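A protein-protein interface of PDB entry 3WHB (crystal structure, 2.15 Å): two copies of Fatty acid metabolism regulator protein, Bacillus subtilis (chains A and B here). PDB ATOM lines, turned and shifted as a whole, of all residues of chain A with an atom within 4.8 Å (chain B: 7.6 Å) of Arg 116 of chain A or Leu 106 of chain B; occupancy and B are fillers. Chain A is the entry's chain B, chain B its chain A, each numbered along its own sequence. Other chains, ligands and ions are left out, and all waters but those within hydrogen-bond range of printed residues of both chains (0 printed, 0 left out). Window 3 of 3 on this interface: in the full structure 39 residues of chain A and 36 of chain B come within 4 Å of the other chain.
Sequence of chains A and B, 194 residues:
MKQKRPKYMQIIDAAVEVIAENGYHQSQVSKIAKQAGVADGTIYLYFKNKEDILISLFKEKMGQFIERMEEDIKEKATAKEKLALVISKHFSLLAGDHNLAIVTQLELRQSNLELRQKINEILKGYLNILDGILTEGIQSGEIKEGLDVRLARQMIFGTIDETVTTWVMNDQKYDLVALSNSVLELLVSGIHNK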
ATOM      1  N   ARG A 109       5.433  19.038  -5.412  1.00  0.00           N
ATOM      2  CA  ARG A 109       5.261  20.090  -4.421  1.00  0.00           C
ATOM      3  C   ARG A 109       4.066  19.754  -3.535  1.00  0.00           C
ATOM      4  O   ARG A 109       2.915  19.921  -3.935  1.00  0.00           O
ATOM      5  CB  ARG A 109       5.103  21.465  -5.095  1.00  0.00           C
ATOM      6  CG  ARG A 109       6.167  21.793  -6.143  1.00  0.00           C
ATOM      7  CD  ARG A 109       7.559  21.928  -5.532  1.00  0.00           C
ATOM      8  NE  ARG A 109       8.603  22.073  -6.553  1.00  0.00           N
ATOM      9  CZ  ARG A 109       9.869  22.411  -6.307  1.00  0.00           C
ATOM     10  NH1 ARG A 109      10.727  22.515  -7.311  1.00  0.00           N
ATOM     11  NH2 ARG A 109      10.280  22.653  -5.065  1.00  0.00           N
ATOM     12  N   GLN A 110       4.354  19.249  -2.342  1.00  0.00           N
ATOM     13  CA  GLN A 110       3.312  18.815  -1.418  1.00  0.00           C
ATOM     14  C   GLN A 110       2.962  19.881  -0.393  1.00  0.00           C
ATOM     15  O   GLN A 110       3.830  20.625   0.066  1.00  0.00           O
ATOM     16  CB  GLN A 110       3.717  17.512  -0.723  1.00  0.00           C
ATOM     17  CG  GLN A 110       3.781  16.318  -1.665  1.00  0.00           C
ATOM     18  CD  GLN A 110       2.422  15.912  -2.209  1.00  0.00           C
ATOM     19  OE1 GLN A 110       1.390  16.144  -1.574  1.00  0.00           O
ATOM     20  NE2 GLN A 110       2.416  15.288  -3.381  1.00  0.00           N
ATOM     21  N   SER A 111       1.678  19.947  -0.049  1.00  0.00           N
ATOM     22  CA  SER A 111       1.174  20.906   0.927  1.00  0.00           C
ATOM     23  C   SER A 111       1.615  20.547   2.348  1.00  0.00           C
ATOM     24  O   SER A 111       2.105  21.404   3.087  1.00  0.00           O
ATOM     25  CB  SER A 111      -0.351  20.988   0.847  1.00  0.00           C
ATOM     26  OG  SER A 111      -0.864  21.836   1.855  1.00  0.00           O
ATOM     27  N   ASN A 112       1.437  19.280   2.719  1.00  0.00           N
ATOM     28  CA  ASN A 112       1.867  18.790   4.025  1.00  0.00           C
ATOM     29  C   ASN A 112       3.374  18.952   4.203  1.00  0.00           C
ATOM     30  O   ASN A 112       4.159  18.520   3.351  1.00  0.00           O
ATOM     31  CB  ASN A 112       1.468  17.330   4.218  1.00  0.00           C
ATOM     32  CG  ASN A 112       1.910  16.786   5.561  1.00  0.00           C
ATOM     33  OD1 ASN A 112       2.985  16.191   5.677  1.00  0.00           O
ATOM     34  ND2 ASN A 112       1.095  17.013   6.591  1.00  0.00           N
ATOM     35  N   LEU A 113       3.759  19.564   5.321  1.00  0.00           N
ATOM     36  CA  LEU A 113       5.136  19.993   5.547  1.00  0.00           C
ATOM     37  C   LEU A 113       6.148  18.845   5.576  1.00  0.00           C
ATOM     38  O   LEU A 113       7.172  18.909   4.894  1.00  0.00           O
ATOM     39  CB  LEU A 113       5.234  20.851   6.820  1.00  0.00           C
ATOM     40  CG  LEU A 113       6.595  21.416   7.256  1.00  0.00           C
ATOM     41  CD1 LEU A 113       7.313  22.167   6.139  1.00  0.00           C
ATOM     42  CD2 LEU A 113       6.437  22.305   8.486  1.00  0.00           C
ATOM     43  N   GLU A 114       5.864  17.804   6.355  1.00  0.00           N
ATOM     44  CA  GLU A 114       6.836  16.723   6.526  1.00  0.00           C
ATOM     45  C   GLU A 114       6.934  15.811   5.294  1.00  0.00           C
ATOM     46  O   GLU A 114       8.012  15.297   4.978  1.00  0.00           O
ATOM     47  CB  GLU A 114       6.608  15.949   7.836  1.00  0.00           C
ATOM     48  CG  GLU A 114       5.219  15.368   8.022  1.00  0.00           C
ATOM     49  CD  GLU A 114       5.079  13.985   7.419  1.00  0.00           C
ATOM     50  OE1 GLU A 114       3.954  13.439   7.455  1.00  0.00           O
ATOM     51  OE2 GLU A 114       6.091  13.442   6.922  1.00  0.00           O
ATOM     52  N   LEU A 115       5.809  15.628   4.605  1.00  0.00           N
ATOM     53  CA  LEU A 115       5.797  15.000   3.292  1.00  0.00           C
ATOM     54  C   LEU A 115       6.597  15.841   2.291  1.00  0.00           C
ATOM     55  O   LEU A 115       7.412  15.304   1.542  1.00  0.00           O
ATOM     56  CB  LEU A 115       4.360  14.803   2.805  1.00  0.00           C
ATOM     57  CG  LEU A 115       4.116  14.129   1.454  1.00  0.00           C
ATOM     58  CD1 LEU A 115       4.813  12.778   1.365  1.00  0.00           C
ATOM     59  CD2 LEU A 115       2.622  13.984   1.206  1.00  0.00           C
ATOM     60  N   ARG A 116       6.374  17.157   2.302  1.00  0.00           N
ATOM     61  CA  ARG A 116       7.126  18.074   1.441  1.00  0.00           C
ATOM     62  C   ARG A 116       8.626  18.018   1.722  1.00  0.00           C
ATOM     63  O   ARG A 116       9.434  18.051   0.795  1.00  0.00           O
ATOM     64  CB  ARG A 116       6.628  19.513   1.584  1.00  0.00           C
ATOM     65  CG  ARG A 116       7.461  20.517   0.797  1.00  0.00           C
ATOM     66  CD  ARG A 116       6.719  21.819   0.578  1.00  0.00           C
ATOM     67  NE  ARG A 116       6.738  22.697   1.746  1.00  0.00           N
ATOM     68  CZ  ARG A 116       5.682  22.948   2.511  1.00  0.00           C
ATOM     69  NH1 ARG A 116       4.514  22.386   2.242  1.00  0.00           N
ATOM     70  NH2 ARG A 116       5.797  23.768   3.548  1.00  0.00           N
ATOM     71  N   GLN A 117       8.982  17.943   3.004  1.00  0.00           N
ATOM     72  CA  GLN A 117      10.375  17.864   3.433  1.00  0.00           C
ATOM     73  C   GLN A 117      11.075  16.611   2.912  1.00  0.00           C
ATOM     74  O   GLN A 117      12.216  16.681   2.466  1.00  0.00           O
ATOM     75  CB  GLN A 117      10.474  17.912   4.957  1.00  0.00           C
ATOM     76  CG  GLN A 117      10.386  19.312   5.545  1.00  0.00           C
ATOM     77  CD  GLN A 117      10.702  19.353   7.033  1.00  0.00           C
ATOM     78  OE1 GLN A 117      10.444  20.354   7.707  1.00  0.00           O
ATOM     79  NE2 GLN A 117      11.270  18.267   7.552  1.00  0.00           N
ATOM     80  N   LYS A 118      10.379  15.477   2.984  1.00  0.00           N
ATOM     81  CA  LYS A 118      10.896  14.190   2.513  1.00  0.00           C
ATOM     82  C   LYS A 118      11.150  14.152   1.005  1.00  0.00           C
ATOM     83  O   LYS A 118      12.159  13.610   0.553  1.00  0.00           O
ATOM     84  CB  LYS A 118       9.945  13.052   2.912  1.00  0.00           C
ATOM     85  CG  LYS A 118      10.463  12.145   4.021  1.00  0.00           C
ATOM     86  CD  LYS A 118      10.621  12.875   5.343  1.00  0.00           C
ATOM     87  CE  LYS A 118      11.392  12.028   6.342  1.00  0.00           C
ATOM     88  NZ  LYS A 118      11.677  12.809   7.574  1.00  0.00           N
ATOM     89  N   ILE A 119      10.229  14.725   0.240  1.00  0.00           N
ATOM     90  CA  ILE A 119      10.350  14.793  -1.219  1.00  0.00           C
ATOM     91  C   ILE A 119      11.414  15.812  -1.645  1.00  0.00           C
ATOM     92  O   ILE A 119      12.203  15.544  -2.551  1.00  0.00           O
ATOM     93  CB  ILE A 119       8.978  15.072  -1.871  1.00  0.00           C
ATOM     94  CG1 ILE A 119       8.081  13.842  -1.693  1.00  0.00           C
ATOM     95  CG2 ILE A 119       9.116  15.440  -3.348  1.00  0.00           C
ATOM     96  CD1 ILE A 119       6.600  14.114  -1.818  1.00  0.00           C
ATOM     97  N   ASN A 120      11.443  16.967  -0.978  1.00  0.00           N
ATOM     98  CA  ASN A 120      12.485  17.968  -1.207  1.00  0.00           C
ATOM     99  C   ASN A 120      13.877  17.406  -0.949  1.00  0.00           C
ATOM    100  O   ASN A 120      14.820  17.708  -1.682  1.00  0.00           O
ATOM    101  CB  ASN A 120      12.261  19.203  -0.329  1.00  0.00           C
ATOM    102  CG  ASN A 120      11.184  20.128  -0.875  1.00  0.00           C
ATOM    103  OD1 ASN A 120      10.837  21.124  -0.242  1.00  0.00           O
ATOM    104  ND2 ASN A 120      10.654  19.808  -2.045  1.00  0.00           N
ATOM    105  N   ILE B  19      -6.928  28.695   3.105  1.00  0.00           N
ATOM    106  CA  ILE B  19      -6.258  27.707   2.255  1.00  0.00           C
ATOM    107  C   ILE B  19      -4.745  27.705   2.504  1.00  0.00           C
ATOM    108  O   ILE B  19      -4.125  26.643   2.553  1.00  0.00           O
ATOM    109  CB  ILE B  19      -6.610  27.890   0.756  1.00  0.00           C
ATOM    110  CG1 ILE B  19      -8.068  27.482   0.499  1.00  0.00           C
ATOM    111  CG2 ILE B  19      -5.690  27.067  -0.134  1.00  0.00           C
ATOM    112  CD1 ILE B  19      -8.600  27.878  -0.865  1.00  0.00           C
ATOM    113  N   ALA B  20      -4.166  28.887   2.698  1.00  0.00           N
ATOM    114  CA  ALA B  20      -2.738  28.991   3.025  1.00  0.00           C
ATOM    115  C   ALA B  20      -2.431  28.385   4.391  1.00  0.00           C
ATOM    116  O   ALA B  20      -1.429  27.691   4.559  1.00  0.00           O
ATOM    117  CB  ALA B  20      -2.268  30.434   2.972  1.00  0.00           C
ATOM    118  N   TYR B  24      -5.354  23.249   1.025  1.00  0.00           N
ATOM    119  CA  TYR B  24      -6.592  23.246   0.247  1.00  0.00           C
ATOM    120  C   TYR B  24      -7.532  22.097   0.597  1.00  0.00           C
ATOM    121  O   TYR B  24      -8.741  22.291   0.701  1.00  0.00           O
ATOM    122  CB  TYR B  24      -6.288  23.234  -1.255  1.00  0.00           C
ATOM    123  CG  TYR B  24      -7.490  22.930  -2.123  1.00  0.00           C
ATOM    124  CD1 TYR B  24      -8.463  23.899  -2.370  1.00  0.00           C
ATOM    125  CD2 TYR B  24      -7.656  21.668  -2.693  1.00  0.00           C
ATOM    126  CE1 TYR B  24      -9.564  23.621  -3.163  1.00  0.00           C
ATOM    127  CE2 TYR B  24      -8.748  21.383  -3.490  1.00  0.00           C
ATOM    128  CZ  TYR B  24      -9.696  22.362  -3.720  1.00  0.00           C
ATOM    129  OH  TYR B  24     -10.777  22.074  -4.511  1.00  0.00           O
ATOM    130  N   LEU B 100      -0.962  34.415  -0.073  1.00  0.00           N
ATOM    131  CA  LEU B 100      -1.125  34.278  -1.516  1.00  0.00           C
ATOM    132  C   LEU B 100       0.028  33.479  -2.134  1.00  0.00           C
ATOM    133  O   LEU B 100      -0.190  32.652  -3.019  1.00  0.00           O
ATOM    134  CB  LEU B 100      -1.212  35.653  -2.179  1.00  0.00           C
ATOM    135  CG  LEU B 100      -1.467  35.659  -3.689  1.00  0.00           C
ATOM    136  CD1 LEU B 100      -2.754  34.905  -4.034  1.00  0.00           C
ATOM    137  CD2 LEU B 100      -1.483  37.080  -4.234  1.00  0.00           C
ATOM    138  N   ALA B 101       1.241  33.719  -1.645  1.00  0.00           N
ATOM    139  CA  ALA B 101       2.434  33.017  -2.136  1.00  0.00           C
ATOM    140  C   ALA B 101       2.365  31.524  -1.835  1.00  0.00           C
ATOM    141  O   ALA B 101       2.765  30.709  -2.653  1.00  0.00           O
ATOM    142  CB  ALA B 101       3.697  33.624  -1.548  1.00  0.00           C
ATOM    143  N   ILE B 102       1.847  31.165  -0.663  1.00  0.00           N
ATOM    144  CA  ILE B 102       1.678  29.752  -0.328  1.00  0.00           C
ATOM    145  C   ILE B 102       0.640  29.113  -1.253  1.00  0.00           C
ATOM    146  O   ILE B 102       0.826  27.991  -1.721  1.00  0.00           O
ATOM    147  CB  ILE B 102       1.347  29.548   1.165  1.00  0.00           C
ATOM    148  CG1 ILE B 102       2.631  29.683   1.992  1.00  0.00           C
ATOM    149  CG2 ILE B 102       0.703  28.182   1.408  1.00  0.00           C
ATOM    150  CD1 ILE B 102       2.399  30.008   3.454  1.00  0.00           C
ATOM    151  N   VAL B 103      -0.431  29.852  -1.531  1.00  0.00           N
ATOM    152  CA  VAL B 103      -1.489  29.394  -2.426  1.00  0.00           C
ATOM    153  C   VAL B 103      -0.988  29.175  -3.854  1.00  0.00           C
ATOM    154  O   VAL B 103      -1.216  28.110  -4.430  1.00  0.00           O
ATOM    155  CB  VAL B 103      -2.699  30.358  -2.415  1.00  0.00           C
ATOM    156  CG1 VAL B 103      -3.767  29.896  -3.397  1.00  0.00           C
ATOM    157  CG2 VAL B 103      -3.293  30.447  -1.012  1.00  0.00           C
ATOM    158  N   THR B 104      -0.300  30.167  -4.422  1.00  0.00           N
ATOM    159  CA  THR B 104       0.195  30.055  -5.804  1.00  0.00           C
ATOM    160  C   THR B 104       1.236  28.946  -5.971  1.00  0.00           C
ATOM    161  O   THR B 104       1.234  28.243  -6.986  1.00  0.00           O
ATOM    162  CB  THR B 104       0.796  31.372  -6.343  1.00  0.00           C
ATOM    163  OG1 THR B 104       1.809  31.847  -5.447  1.00  0.00           O
ATOM    164  CG2 THR B 104      -0.277  32.440  -6.538  1.00  0.00           C
ATOM    165  N   GLN B 105       2.103  28.792  -4.971  1.00  0.00           N
ATOM    166  CA  GLN B 105       3.247  27.873  -5.069  1.00  0.00           C
ATOM    167  C   GLN B 105       2.947  26.446  -4.606  1.00  0.00           C
ATOM    168  O   GLN B 105       3.643  25.506  -5.008  1.00  0.00           O
ATOM    169  CB  GLN B 105       4.466  28.417  -4.303  1.00  0.00           C
ATOM    170  CG  GLN B 105       4.984  29.774  -4.776  1.00  0.00           C
ATOM    171  CD  GLN B 105       4.996  29.926  -6.289  1.00  0.00           C
ATOM    172  OE1 GLN B 105       4.176  30.649  -6.852  1.00  0.00           O
ATOM    173  NE2 GLN B 105       5.926  29.239  -6.956  1.00  0.00           N
ATOM    174  N   LEU B 106       1.927  26.288  -3.759  1.00  0.00           N
ATOM    175  CA  LEU B 106       1.601  24.981  -3.194  1.00  0.00           C
ATOM    176  C   LEU B 106       0.137  24.580  -3.366  1.00  0.00           C
ATOM    177  O   LEU B 106      -0.168  23.553  -3.980  1.00  0.00           O
ATOM    178  CB  LEU B 106       1.989  24.930  -1.709  1.00  0.00           C
ATOM    179  CG  LEU B 106       3.469  25.110  -1.357  1.00  0.00           C
ATOM    180  CD1 LEU B 106       3.634  25.425   0.126  1.00  0.00           C
ATOM    181  CD2 LEU B 106       4.271  23.881  -1.752  1.00  0.00           C
ATOM    182  N   GLU B 107      -0.766  25.397  -2.835  1.00  0.00           N
ATOM    183  CA  GLU B 107      -2.166  25.001  -2.714  1.00  0.00           C
ATOM    184  C   GLU B 107      -2.926  24.940  -4.041  1.00  0.00           C
ATOM    185  O   GLU B 107      -3.844  24.140  -4.186  1.00  0.00           O
ATOM    186  CB  GLU B 107      -2.886  25.891  -1.700  1.00  0.00           C
ATOM    187  CG  GLU B 107      -2.264  25.887  -0.300  1.00  0.00           C
ATOM    188  CD  GLU B 107      -1.983  24.491   0.238  1.00  0.00           C
ATOM    189  OE1 GLU B 107      -2.778  23.559  -0.020  1.00  0.00           O
ATOM    190  OE2 GLU B 107      -0.958  24.325   0.928  1.00  0.00           O
ATOM    191  N   LEU B 108      -2.533  25.780  -4.995  1.00  0.00           N
ATOM    192  CA  LEU B 108      -3.067  25.725  -6.352  1.00  0.00           C
ATOM    193  C   LEU B 108      -2.462  24.578  -7.161  1.00  0.00           C
ATOM    194  O   LEU B 108      -2.967  24.239  -8.233  1.00  0.00           O
ATOM    195  CB  LEU B 108      -2.830  27.052  -7.087  1.00  0.00           C
ATOM    196  CG  LEU B 108      -3.882  28.163  -6.993  1.00  0.00           C
ATOM    197  CD1 LEU B 108      -3.290  29.489  -7.445  1.00  0.00           C
ATOM    198  CD2 LEU B 108      -5.119  27.839  -7.813  1.00  0.00           C
ATOM    199  N   ARG B 109      -1.384  23.984  -6.653  1.00  0.00           N
ATOM    200  CA  ARG B 109      -0.700  22.893  -7.364  1.00  0.00           C
ATOM    201  C   ARG B 109      -1.398  21.565  -7.089  1.00  0.00           C
ATOM    202  O   ARG B 109      -0.806  20.635  -6.517  1.00  0.00           O
ATOM    203  CB  ARG B 109       0.783  22.819  -6.985  1.00  0.00           C
ATOM    204  CG  ARG B 109       1.476  24.167  -6.914  1.00  0.00           C
ATOM    205  CD  ARG B 109       2.205  24.534  -8.194  1.00  0.00           C
ATOM    206  NE  ARG B 109       2.390  25.982  -8.279  1.00  0.00           N
ATOM    207  CZ  ARG B 109       3.420  26.593  -8.860  1.00  0.00           C
ATOM    208  NH1 ARG B 109       4.405  25.890  -9.410  1.00  0.00           N
ATOM    209  NH2 ARG B 109       3.470  27.917  -8.874  1.00  0.00           N
ATOM    210  N   GLN B 110      -2.666  21.500  -7.493  1.00  0.00           N
ATOM    211  CA  GLN B 110      -3.489  20.302  -7.354  1.00  0.00           C
ATOM    212  C   GLN B 110      -3.110  19.269  -8.399  1.00  0.00           C
ATOM    213  O   GLN B 110      -2.772  19.611  -9.537  1.00  0.00           O
ATOM    214  CB  GLN B 110      -4.978  20.647  -7.462  1.00  0.00           C
ATOM    215  CG  GLN B 110      -5.500  21.492  -6.309  1.00  0.00           C
ATOM    216  CD  GLN B 110      -5.178  20.896  -4.949  1.00  0.00           C
ATOM    217  OE1 GLN B 110      -5.544  19.758  -4.647  1.00  0.00           O
ATOM    218  NE2 GLN B 110      -4.491  21.668  -4.118  1.00  0.00           N
ATOM    219  N   SER B 111      -3.170  18.004  -8.000  1.00  0.00           N
ATOM    220  CA  SER B 111      -2.742  16.908  -8.854  1.00  0.00           C
ATOM    221  C   SER B 111      -3.905  16.224  -9.554  1.00  0.00           C
ATOM    222  O   SER B 111      -3.696  15.313 -10.361  1.00  0.00           O
ATOM    223  CB  SER B 111      -1.935  15.893  -8.053  1.00  0.00           C
ATOM    224  OG  SER B 111      -2.707  15.323  -7.009  1.00  0.00           O
ATOM    225  N   ARG B 116      -6.610  20.822 -12.559  1.00  0.00           N
ATOM    226  CA  ARG B 116      -5.389  21.504 -12.958  1.00  0.00           C
ATOM    227  C   ARG B 116      -5.455  22.055 -14.393  1.00  0.00           C
ATOM    228  O   ARG B 116      -4.706  22.977 -14.737  1.00  0.00           O
ATOM    229  CB  ARG B 116      -4.192  20.569 -12.765  1.00  0.00           C
ATOM    230  CG  ARG B 116      -2.829  21.226 -12.879  1.00  0.00           C
ATOM    231  CD  ARG B 116      -2.436  22.051 -11.663  1.00  0.00           C
ATOM    232  NE  ARG B 116      -1.029  22.435 -11.766  1.00  0.00           N
ATOM    233  CZ  ARG B 116      -0.022  21.797 -11.175  1.00  0.00           C
ATOM    234  NH1 ARG B 116       1.226  22.223 -11.353  1.00  0.00           N
ATOM    235  NH2 ARG B 116      -0.251  20.743 -10.402  1.00  0.00           N
ATOM    236  N   THR B 165       9.144  29.516  -5.665  1.00  0.00           N
ATOM    237  CA  THR B 165       8.982  28.262  -4.930  1.00  0.00           C
ATOM    238  C   THR B 165      10.117  28.053  -3.927  1.00  0.00           C
ATOM    239  O   THR B 165       9.858  27.802  -2.749  1.00  0.00           O
ATOM    240  CB  THR B 165       8.860  27.053  -5.877  1.00  0.00           C
ATOM    241  OG1 THR B 165       7.682  27.208  -6.665  1.00  0.00           O
ATOM    242  CG2 THR B 165       8.775  25.744  -5.096  1.00  0.00           C
ATOM    243  N   VAL B 168       9.600  30.233  -1.075  1.00  0.00           N
ATOM    244  CA  VAL B 168       8.508  29.725  -0.236  1.00  0.00           C
ATOM    245  C   VAL B 168       8.972  28.540   0.608  1.00  0.00           C
ATOM    246  O   VAL B 168       8.658  28.469   1.795  1.00  0.00           O
ATOM    247  CB  VAL B 168       7.228  29.380  -1.048  1.00  0.00           C
ATOM    248  CG1 VAL B 168       6.262  28.531  -0.227  1.00  0.00           C
ATOM    249  CG2 VAL B 168       6.530  30.651  -1.512  1.00  0.00           C
ATOM    250  N   MET B 169       9.751  27.640   0.004  1.00  0.00           N
ATOM    251  CA  MET B 169      10.335  26.503   0.727  1.00  0.00           C
ATOM    252  C   MET B 169      11.211  26.949   1.894  1.00  0.00           C
ATOM    253  O   MET B 169      11.301  26.253   2.906  1.00  0.00           O
ATOM    254  CB  MET B 169      11.163  25.608  -0.207  1.00  0.00           C
ATOM    255  CG  MET B 169      10.357  24.831  -1.233  1.00  0.00           C
ATOM    256  SD  MET B 169       8.882  24.046  -0.554  1.00  0.00           S
ATOM    257  CE  MET B 169       8.382  23.124  -2.010  1.00  0.00           C
ATOM    258  N   ASN B 170      11.864  28.099   1.738  1.00  0.00           N
ATOM    259  CA  ASN B 170      12.684  28.668   2.802  1.00  0.00           C
ATOM    260  C   ASN B 170      11.924  29.709   3.628  1.00  0.00           C
ATOM    261  O   ASN B 170      12.503  30.690   4.095  1.00  0.00           O
ATOM    262  CB  ASN B 170      13.982  29.245   2.221  1.00  0.00           C
ATOM    263  CG  ASN B 170      14.907  28.165   1.705  1.00  0.00           C
ATOM    264  OD1 ASN B 170      15.645  27.550   2.470  1.00  0.00           O
ATOM    265  ND2 ASN B 170      14.860  27.917   0.400  1.00  0.00           N
ATOM    266  N   ASP B 171      10.616  29.488   3.774  1.00  0.00           N
ATOM    267  CA  ASP B 171       9.749  30.290   4.648  1.00  0.00           C
ATOM    268  C   ASP B 171       9.711  31.779   4.313  1.00  0.00           C
ATOM    269  O   ASP B 171       9.393  32.606   5.168  1.00  0.00           O
ATOM    270  CB  ASP B 171      10.130  30.078   6.119  1.00  0.00           C
ATOM    271  CG  ASP B 171       9.520  28.823   6.696  1.00  0.00           C
ATOM    272  OD1 ASP B 171      10.269  27.853   6.930  1.00  0.00           O
ATOM    273  OD2 ASP B 171       8.286  28.799   6.899  1.00  0.00           O
ATOM    274  N   GLN B 172      10.038  32.106   3.064  1.00  0.00           N
ATOM    275  CA  GLN B 172       9.972  33.475   2.557  1.00  0.00           C
ATOM    276  C   GLN B 172      10.814  34.420   3.408  1.00  0.00           C
ATOM    277  O   GLN B 172      10.424  35.558   3.666  1.00  0.00           O
ATOM    278  CB  GLN B 172       8.512  33.941   2.520  1.00  0.00           C
ATOM    279  CG  GLN B 172       7.567  32.954   1.843  1.00  0.00           C
ATOM    280  CD  GLN B 172       6.117  33.385   1.897  1.00  0.00           C
ATOM    281  OE1 GLN B 172       5.807  34.576   1.962  1.00  0.00           O
ATOM    282  NE2 GLN B 172       5.216  32.418   1.856  1.00  0.00           N
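Of the printed residues of chain B, Gln 110 of chain A touches Leu 106. Of the printed residues of chain B, Ser 111 of chain A touches Glu 107 (2.7 Å). Asn 112 of chain A touches none of the printed residues of chain B. Leu 115 of chain A touches none of the printed residues of chain B. Arg 116 of chain A touches just these residues of chain B: Leu 106 and Met 169. Of the printed residues of chain B, Asn 120 of chain A touches Met 169 (3.5 Å). Of the printed residues of chain A, Glu 107 of chain B touches Ser 111. Of the printed residues of chain A, Met 169 of chain B touches Arg 109 (3.6 Å), Arg 116 (3.3 Å) and Asn 120 (3.5 Å). The nearest residue of chain B that does not touch Arg 116 of chain A is Val 168 of chain B (5.8 Å). The nearest printed residue of chain B that does not touch Asn 120 of chain A is Thr 165 of chain B (6.9 Å).
Among the printed residues, merely in contact across the chains: Arg 109 of chain A with Thr 165 of chain B (3.4 Å), Arg 109 of chain A with Met 169 of chain B (3.6 Å), Gln 110 of chain A with Leu 106 of chain B (3.8 Å) and Arg 116 of chain A with Leu 106 of chain B (3.8 Å).
Positions printed for both chains: 109, 110, 111 and 116.
Of the 22 printed residues of chain B, 4 touch a printed residue of chain A. Hydrophobic or aromatic side chains of chain B within 4 Å of the printed part of chain A: Leu 106 and Met 169. Along chain B the printed residues that touch a printed residue of chain A span positions 106 to 169. Among the printed residues, 7 pairs touch across the chains. Among the printed residues, no Asp or Glu carboxylate lies within 4 Å of a Lys or Arg side-chain nitrogen of the other chain.
The side-chain hydroxyl (OG) of Ser 111 of chain A lies within hydrogen-bond range of the side-chain carboxylate (OE2) of Glu 107 of chain B (2.7 Å). The side-chain sulfur (SD) of Met 169 of chain B sits close to the side-chain amide oxygen (OD1) of Asn 120 of chain A (3.5 Å). The side-chain sulfur of Met 169 of chain B sits close to the guanidinium group of Arg 116 of chain A.
O of Gln 110 of chain A lies within hydrogen-bond range of NH1 of Arg 116 of chain A, 2.9 Å away. The side-chain amide nitrogen (NE2) of Gln 105 of chain B is in hydrogen-bond range of the side-chain hydroxyl (OG1) of Thr 165 of chain B (2.7 Å). O of Glu 107 of chain B sits at hydrogen-bond distance from NE2 of Gln 110 of chain B, 2.6 Å away. N of Tyr 24 of chain B is in hydrogen-bond range of OE1 of Glu 107 of chain B (2.8 Å). The backbone NH (N) of Glu 107 of chain B is in hydrogen-bond range of the backbone carbonyl oxygen (O) of Ile 102 of chain B, 3.2 Å away. The backbone carbonyl oxygen (O) of Ser 111 of chain A is in hydrogen-bond range of the guanidinium group (NH1) of Arg 116 of chain A, at 2.7 Å.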
